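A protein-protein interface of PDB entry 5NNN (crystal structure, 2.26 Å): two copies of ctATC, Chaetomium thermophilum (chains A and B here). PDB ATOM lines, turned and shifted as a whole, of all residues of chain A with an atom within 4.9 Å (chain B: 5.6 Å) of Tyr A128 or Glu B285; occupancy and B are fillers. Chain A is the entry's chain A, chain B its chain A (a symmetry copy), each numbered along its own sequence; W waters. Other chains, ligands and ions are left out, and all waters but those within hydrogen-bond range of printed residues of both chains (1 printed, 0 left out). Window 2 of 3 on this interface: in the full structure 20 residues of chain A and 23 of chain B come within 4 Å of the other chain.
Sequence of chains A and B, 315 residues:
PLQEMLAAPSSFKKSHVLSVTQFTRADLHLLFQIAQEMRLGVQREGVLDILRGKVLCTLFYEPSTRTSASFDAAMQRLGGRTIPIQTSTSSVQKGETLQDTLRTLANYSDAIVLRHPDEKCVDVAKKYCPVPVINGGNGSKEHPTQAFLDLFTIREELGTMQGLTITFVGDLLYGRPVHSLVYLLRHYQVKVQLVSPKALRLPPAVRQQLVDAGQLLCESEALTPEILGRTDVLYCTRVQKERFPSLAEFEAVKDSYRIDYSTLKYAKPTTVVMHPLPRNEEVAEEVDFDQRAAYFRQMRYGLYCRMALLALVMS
Among the printed residues, merely in contact across the chains: Arg A103 with Arg B279 (3.6 Å) and Lys A127 with Phe B289 (3.6 Å).
The side-chain hydroxyl of Tyr A128 sits at hydrogen-bond distance from the side-chain carboxylate of Glu B285 (3.1 Å). NE2 of Gln A99 sits at hydrogen-bond distance from OE2 of Glu B285, 3.0 Å away. NH1 of Arg A103 lies within salt-bridge range of OD2 of Asp B288.
Of the printed residues of chain B, Tyr A128 touches Glu B285. Of the printed residues of chain A, Glu B285 touches Gln A99 and Tyr A128. Of the printed residues of chain A, Asp B288 touches Arg A103. Printed residues of chain B within 4 Å of Arg A103: Arg B279 (3.6 Å) and Asp B288 (2.8 Å). Lys A126 touches none of the printed residues of chain B. The nearest printed residue of chain B that does not touch Lys A127 is Glu B285 (5.5 Å).
Of the 10 printed residues of chain B, 4 touch a printed residue of chain A. Hydrophobic or aromatic side chains of chain B that line the printed part of chain A: Phe B289. Among the printed residues, Asp or Glu carboxylates within 4 Å of a Lys or Arg side-chain nitrogen of the other chain: Arg A103 with Asp B288 (2.8 Å).
Water W1 bridges the side-chain carboxylate of Glu B285 (2.7 Å) and the side-chain hydroxyl of Thr A97 (3.3 Å).
No position is printed for both chains.
The backbone carbonyl oxygen (O) of Gln A99 lies within hydrogen-bond range of the guanidinium group (NE) of Arg A103. OD1 of Asp B288 is in hydrogen-bond range of OH of Tyr B295 (2.7 Å). The guanidinium group of Arg B279 is in salt-bridge range of the side-chain carboxylate of Asp B288 (2.7 Å). The backbone carbonyl oxygen of Val B283 lies within hydrogen-bond range of the guanidinium group of Arg B279 (2.9 Å). The side-chain amino group of Lys A127 is in hydrogen-bond range of the side-chain hydroxyl of Tyr A128, 3.0 Å away.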
ATOM      1  N   THR A  97      24.048 -28.197  -9.448  1.00  0.00           N
ATOM      2  CA  THR A  97      22.639 -28.479  -9.325  1.00  0.00           C
ATOM      3  C   THR A  97      21.875 -27.752 -10.415  1.00  0.00           C
ATOM      4  O   THR A  97      22.322 -26.747 -10.991  1.00  0.00           O
ATOM      5  CB  THR A  97      22.084 -28.051  -7.951  1.00  0.00           C
ATOM      6  OG1 THR A  97      22.245 -26.646  -7.822  1.00  0.00           O
ATOM      7  CG2 THR A  97      22.807 -28.727  -6.799  1.00  0.00           C
ATOM      8  N   GLN A  99      19.081 -26.010 -10.000  1.00  0.00           N
ATOM      9  CA  GLN A  99      18.668 -24.643  -9.640  1.00  0.00           C
ATOM     10  C   GLN A  99      19.811 -23.653  -9.826  1.00  0.00           C
ATOM     11  O   GLN A  99      19.586 -22.516 -10.278  1.00  0.00           O
ATOM     12  CB  GLN A  99      18.122 -24.589  -8.208  1.00  0.00           C
ATOM     13  CG  GLN A  99      19.040 -25.218  -7.149  1.00  0.00           C
ATOM     14  CD  GLN A  99      18.644 -26.634  -6.840  1.00  0.00           C
ATOM     15  OE1 GLN A  99      18.554 -27.526  -7.728  1.00  0.00           O
ATOM     16  NE2 GLN A  99      18.405 -26.864  -5.577  1.00  0.00           N
ATOM     17  N   ARG A 103      19.580 -20.588 -12.570  1.00  0.00           N
ATOM     18  CA  ARG A 103      19.829 -19.196 -12.203  1.00  0.00           C
ATOM     19  C   ARG A 103      21.045 -18.646 -12.934  1.00  0.00           C
ATOM     20  O   ARG A 103      21.043 -17.492 -13.350  1.00  0.00           O
ATOM     21  CB  ARG A 103      19.934 -19.106 -10.684  1.00  0.00           C
ATOM     22  CG  ARG A 103      18.481 -19.151  -9.963  1.00  0.00           C
ATOM     23  CD  ARG A 103      18.603 -19.330  -8.460  1.00  0.00           C
ATOM     24  NE  ARG A 103      19.271 -20.572  -8.092  1.00  0.00           N
ATOM     25  CZ  ARG A 103      19.449 -20.988  -6.849  1.00  0.00           C
ATOM     26  NH1 ARG A 103      18.970 -20.271  -5.828  1.00  0.00           N
ATOM     27  NH2 ARG A 103      20.068 -22.150  -6.614  1.00  0.00           N
ATOM     28  N   VAL A 124      11.458 -27.342  -9.310  1.00  0.00           N
ATOM     29  CA  VAL A 124      12.691 -26.588  -9.147  1.00  0.00           C
ATOM     30  C   VAL A 124      12.623 -25.344  -9.996  1.00  0.00           C
ATOM     31  O   VAL A 124      12.898 -24.239  -9.519  1.00  0.00           O
ATOM     32  CB  VAL A 124      13.908 -27.486  -9.487  1.00  0.00           C
ATOM     33  CG1 VAL A 124      15.203 -26.705  -9.452  1.00  0.00           C
ATOM     34  CG2 VAL A 124      14.024 -28.612  -8.464  1.00  0.00           C
ATOM     35  N   ALA A 125      12.152 -25.480 -11.249  1.00  0.00           N
ATOM     36  CA  ALA A 125      12.192 -24.321 -12.141  1.00  0.00           C
ATOM     37  C   ALA A 125      11.246 -23.247 -11.653  1.00  0.00           C
ATOM     38  O   ALA A 125      11.477 -22.049 -11.882  1.00  0.00           O
ATOM     39  CB  ALA A 125      11.794 -24.712 -13.574  1.00  0.00           C
ATOM     40  N   LYS A 126      10.155 -23.675 -11.026  1.00  0.00           N
ATOM     41  CA  LYS A 126       9.167 -22.724 -10.563  1.00  0.00           C
ATOM     42  C   LYS A 126       9.696 -21.994  -9.336  1.00  0.00           C
ATOM     43  O   LYS A 126       9.651 -20.767  -9.288  1.00  0.00           O
ATOM     44  CB  LYS A 126       7.834 -23.449 -10.281  1.00  0.00           C
ATOM     45  CG  LYS A 126       6.612 -22.504 -10.278  1.00  0.00           C
ATOM     46  CD  LYS A 126       5.294 -23.212  -9.910  1.00  0.00           C
ATOM     47  CE  LYS A 126       4.168 -22.183  -9.640  1.00  0.00           C
ATOM     48  NZ  LYS A 126       3.795 -21.302 -10.817  1.00  0.00           N
ATOM     49  N   LYS A 127      10.292 -22.730  -8.385  1.00  0.00           N
ATOM     50  CA  LYS A 127      10.836 -22.089  -7.182  1.00  0.00           C
ATOM     51  C   LYS A 127      12.013 -21.143  -7.444  1.00  0.00           C
ATOM     52  O   LYS A 127      12.178 -20.187  -6.689  1.00  0.00           O
ATOM     53  CB  LYS A 127      11.298 -23.156  -6.206  1.00  0.00           C
ATOM     54  CG  LYS A 127      11.792 -22.599  -4.861  1.00  0.00           C
ATOM     55  CD  LYS A 127      11.872 -23.743  -3.861  1.00  0.00           C
ATOM     56  CE  LYS A 127      12.626 -23.378  -2.583  1.00  0.00           C
ATOM     57  NZ  LYS A 127      13.345 -24.579  -2.023  1.00  0.00           N
ATOM     58  N   TYR A 128      12.875 -21.384  -8.476  1.00  0.00           N
ATOM     59  CA  TYR A 128      14.170 -20.708  -8.502  1.00  0.00           C
ATOM     60  C   TYR A 128      14.422 -19.855  -9.725  1.00  0.00           C
ATOM     61  O   TYR A 128      15.152 -18.868  -9.623  1.00  0.00           O
ATOM     62  CB  TYR A 128      15.306 -21.724  -8.385  1.00  0.00           C
ATOM     63  CG  TYR A 128      15.470 -22.318  -7.043  1.00  0.00           C
ATOM     64  CD1 TYR A 128      15.961 -21.560  -6.007  1.00  0.00           C
ATOM     65  CD2 TYR A 128      15.135 -23.651  -6.791  1.00  0.00           C
ATOM     66  CE1 TYR A 128      16.129 -22.112  -4.747  1.00  0.00           C
ATOM     67  CE2 TYR A 128      15.276 -24.194  -5.538  1.00  0.00           C
ATOM     68  CZ  TYR A 128      15.795 -23.399  -4.513  1.00  0.00           C
ATOM     69  OH  TYR A 128      15.965 -23.904  -3.243  1.00  0.00           O
ATOM     70  N   CYS A 129      13.840 -20.163 -10.814  1.00  0.00           N
ATOM     71  CA  CYS A 129      14.230 -19.574 -12.073  1.00  0.00           C
ATOM     72  C   CYS A 129      13.449 -18.279 -12.311  1.00  0.00           C
ATOM     73  O   CYS A 129      12.217 -18.302 -12.301  1.00  0.00           O
ATOM     74  CB  CYS A 129      13.983 -20.548 -13.255  1.00  0.00           C
ATOM     75  SG  CYS A 129      14.671 -19.931 -14.841  1.00  0.00           S
ATOM     76  N   PRO A 130      14.134 -17.177 -12.577  1.00  0.00           N
ATOM     77  CA  PRO A 130      13.462 -15.876 -12.727  1.00  0.00           C
ATOM     78  C   PRO A 130      13.114 -15.527 -14.155  1.00  0.00           C
ATOM     79  O   PRO A 130      12.936 -14.349 -14.425  1.00  0.00           O
ATOM     80  CB  PRO A 130      14.516 -14.886 -12.193  1.00  0.00           C
ATOM     81  CG  PRO A 130      15.874 -15.569 -12.627  1.00  0.00           C
ATOM     82  CD  PRO A 130      15.615 -17.041 -12.500  1.00  0.00           C
ATOM     83  N   ARG B 258      31.090 -22.544   6.424  1.00  0.00           N
ATOM     84  CA  ARG B 258      29.813 -22.523   5.728  1.00  0.00           C
ATOM     85  C   ARG B 258      29.081 -21.217   6.014  1.00  0.00           C
ATOM     86  O   ARG B 258      28.872 -20.856   7.172  1.00  0.00           O
ATOM     87  CB  ARG B 258      28.985 -23.728   6.171  1.00  0.00           C
ATOM     88  CG  ARG B 258      27.694 -23.918   5.417  1.00  0.00           C
ATOM     89  CD  ARG B 258      27.143 -25.336   5.585  1.00  0.00           C
ATOM     90  NE  ARG B 258      25.666 -25.392   5.543  1.00  0.00           N
ATOM     91  CZ  ARG B 258      24.913 -25.569   4.445  1.00  0.00           C
ATOM     92  NH1 ARG B 258      25.458 -25.705   3.236  1.00  0.00           N
ATOM     93  NH2 ARG B 258      23.585 -25.607   4.556  1.00  0.00           N
ATOM     94  N   ARG B 279      29.722 -23.998  -6.568  1.00  0.00           N
ATOM     95  CA  ARG B 279      29.855 -24.163  -5.128  1.00  0.00           C
ATOM     96  C   ARG B 279      29.472 -25.588  -4.749  1.00  0.00           C
ATOM     97  O   ARG B 279      28.676 -26.223  -5.448  1.00  0.00           O
ATOM     98  CB  ARG B 279      28.929 -23.183  -4.373  1.00  0.00           C
ATOM     99  CG  ARG B 279      27.420 -23.374  -4.736  1.00  0.00           C
ATOM    100  CD  ARG B 279      26.404 -22.847  -3.669  1.00  0.00           C
ATOM    101  NE  ARG B 279      25.125 -22.586  -4.335  1.00  0.00           N
ATOM    102  CZ  ARG B 279      24.071 -21.992  -3.808  1.00  0.00           C
ATOM    103  NH1 ARG B 279      24.071 -21.571  -2.545  1.00  0.00           N
ATOM    104  NH2 ARG B 279      23.016 -21.826  -4.567  1.00  0.00           N
ATOM    105  N   VAL B 283      28.261 -22.339   0.641  1.00  0.00           N
ATOM    106  CA  VAL B 283      27.198 -21.346   0.796  1.00  0.00           C
ATOM    107  C   VAL B 283      25.865 -22.072   0.756  1.00  0.00           C
ATOM    108  O   VAL B 283      25.514 -22.693  -0.257  1.00  0.00           O
ATOM    109  CB  VAL B 283      27.266 -20.242  -0.249  1.00  0.00           C
ATOM    110  CG1 VAL B 283      26.087 -19.257  -0.039  1.00  0.00           C
ATOM    111  CG2 VAL B 283      28.562 -19.535  -0.069  1.00  0.00           C
ATOM    112  N   ALA B 284      25.151 -22.032   1.879  1.00  0.00           N
ATOM    113  CA  ALA B 284      23.897 -22.751   2.011  1.00  0.00           C
ATOM    114  C   ALA B 284      22.826 -22.162   1.085  1.00  0.00           C
ATOM    115  O   ALA B 284      22.782 -20.941   0.831  1.00  0.00           O
ATOM    116  CB  ALA B 284      23.424 -22.710   3.470  1.00  0.00           C
ATOM    117  N   GLU B 285      21.975 -23.057   0.568  1.00  0.00           N
ATOM    118  CA  GLU B 285      20.839 -22.655  -0.272  1.00  0.00           C
ATOM    119  C   GLU B 285      19.896 -21.705   0.466  1.00  0.00           C
ATOM    120  O   GLU B 285      19.383 -20.735  -0.132  1.00  0.00           O
ATOM    121  CB  GLU B 285      20.067 -23.891  -0.748  1.00  0.00           C
ATOM    122  CG  GLU B 285      20.834 -24.636  -1.865  1.00  0.00           C
ATOM    123  CD  GLU B 285      19.950 -25.434  -2.854  1.00  0.00           C
ATOM    124  OE1 GLU B 285      18.697 -25.255  -2.914  1.00  0.00           O
ATOM    125  OE2 GLU B 285      20.550 -26.251  -3.599  1.00  0.00           O
ATOM    126  N   GLU B 286      19.729 -21.919   1.787  1.00  0.00           N
ATOM    127  CA  GLU B 286      18.853 -21.073   2.610  1.00  0.00           C
ATOM    128  C   GLU B 286      19.222 -19.600   2.522  1.00  0.00           C
ATOM    129  O   GLU B 286      18.416 -18.749   2.895  1.00  0.00           O
ATOM    130  CB  GLU B 286      18.882 -21.545   4.061  1.00  0.00           C
ATOM    131  CG  GLU B 286      20.068 -21.022   4.912  1.00  0.00           C
ATOM    132  CD  GLU B 286      20.029 -21.541   6.334  1.00  0.00           C
ATOM    133  OE1 GLU B 286      19.039 -22.221   6.682  1.00  0.00           O
ATOM    134  OE2 GLU B 286      20.976 -21.280   7.111  1.00  0.00           O
ATOM    135  N   VAL B 287      20.395 -19.282   1.974  1.00  0.00           N
ATOM    136  CA  VAL B 287      20.864 -17.918   1.879  1.00  0.00           C
ATOM    137  C   VAL B 287      20.659 -17.318   0.497  1.00  0.00           C
ATOM    138  O   VAL B 287      20.839 -16.098   0.329  1.00  0.00           O
ATOM    139  CB  VAL B 287      22.340 -17.915   2.347  1.00  0.00           C
ATOM    140  CG1 VAL B 287      23.198 -16.817   1.729  1.00  0.00           C
ATOM    141  CG2 VAL B 287      22.349 -17.875   3.896  1.00  0.00           C
ATOM    142  N   ASP B 288      20.211 -18.103  -0.482  1.00  0.00           N
ATOM    143  CA  ASP B 288      20.237 -17.626  -1.874  1.00  0.00           C
ATOM    144  C   ASP B 288      19.300 -16.451  -2.115  1.00  0.00           C
ATOM    145  O   ASP B 288      19.503 -15.676  -3.062  1.00  0.00           O
ATOM    146  CB  ASP B 288      19.823 -18.752  -2.841  1.00  0.00           C
ATOM    147  CG  ASP B 288      20.832 -19.917  -2.931  1.00  0.00           C
ATOM    148  OD1 ASP B 288      21.933 -19.879  -2.351  1.00  0.00           O
ATOM    149  OD2 ASP B 288      20.474 -20.911  -3.580  1.00  0.00           O
ATOM    150  N   PHE B 289      18.211 -16.382  -1.377  1.00  0.00           N
ATOM    151  CA  PHE B 289      17.225 -15.334  -1.590  1.00  0.00           C
ATOM    152  C   PHE B 289      17.541 -14.085  -0.788  1.00  0.00           C
ATOM    153  O   PHE B 289      16.863 -13.067  -0.959  1.00  0.00           O
ATOM    154  CB  PHE B 289      15.827 -15.883  -1.258  1.00  0.00           C
ATOM    155  CG  PHE B 289      15.212 -16.633  -2.411  1.00  0.00           C
ATOM    156  CD1 PHE B 289      14.970 -15.973  -3.607  1.00  0.00           C
ATOM    157  CD2 PHE B 289      14.936 -17.986  -2.335  1.00  0.00           C
ATOM    158  CE1 PHE B 289      14.439 -16.644  -4.709  1.00  0.00           C
ATOM    159  CE2 PHE B 289      14.407 -18.651  -3.426  1.00  0.00           C
ATOM    160  CZ  PHE B 289      14.157 -17.952  -4.615  1.00  0.00           C
ATOM    161  N   TYR B 295      26.041 -13.859  -5.734  1.00  0.00           N
ATOM    162  CA  TYR B 295      26.716 -14.767  -6.669  1.00  0.00           C
ATOM    163  C   TYR B 295      25.921 -15.091  -7.937  1.00  0.00           C
ATOM    164  O   TYR B 295      26.512 -15.597  -8.898  1.00  0.00           O
ATOM    165  CB  TYR B 295      27.067 -16.070  -5.970  1.00  0.00           C
ATOM    166  CG  TYR B 295      26.151 -16.555  -4.858  1.00  0.00           C
ATOM    167  CD1 TYR B 295      26.358 -16.156  -3.556  1.00  0.00           C
ATOM    168  CD2 TYR B 295      25.121 -17.466  -5.109  1.00  0.00           C
ATOM    169  CE1 TYR B 295      25.554 -16.618  -2.523  1.00  0.00           C
ATOM    170  CE2 TYR B 295      24.321 -17.944  -4.083  1.00  0.00           C
ATOM    171  CZ  TYR B 295      24.538 -17.492  -2.776  1.00  0.00           C
ATOM    172  OH  TYR B 295      23.744 -17.958  -1.714  1.00  0.00           O
HETATM  173  O   HOH W   1      22.702 -25.341  -4.851  1.00  0.00           O
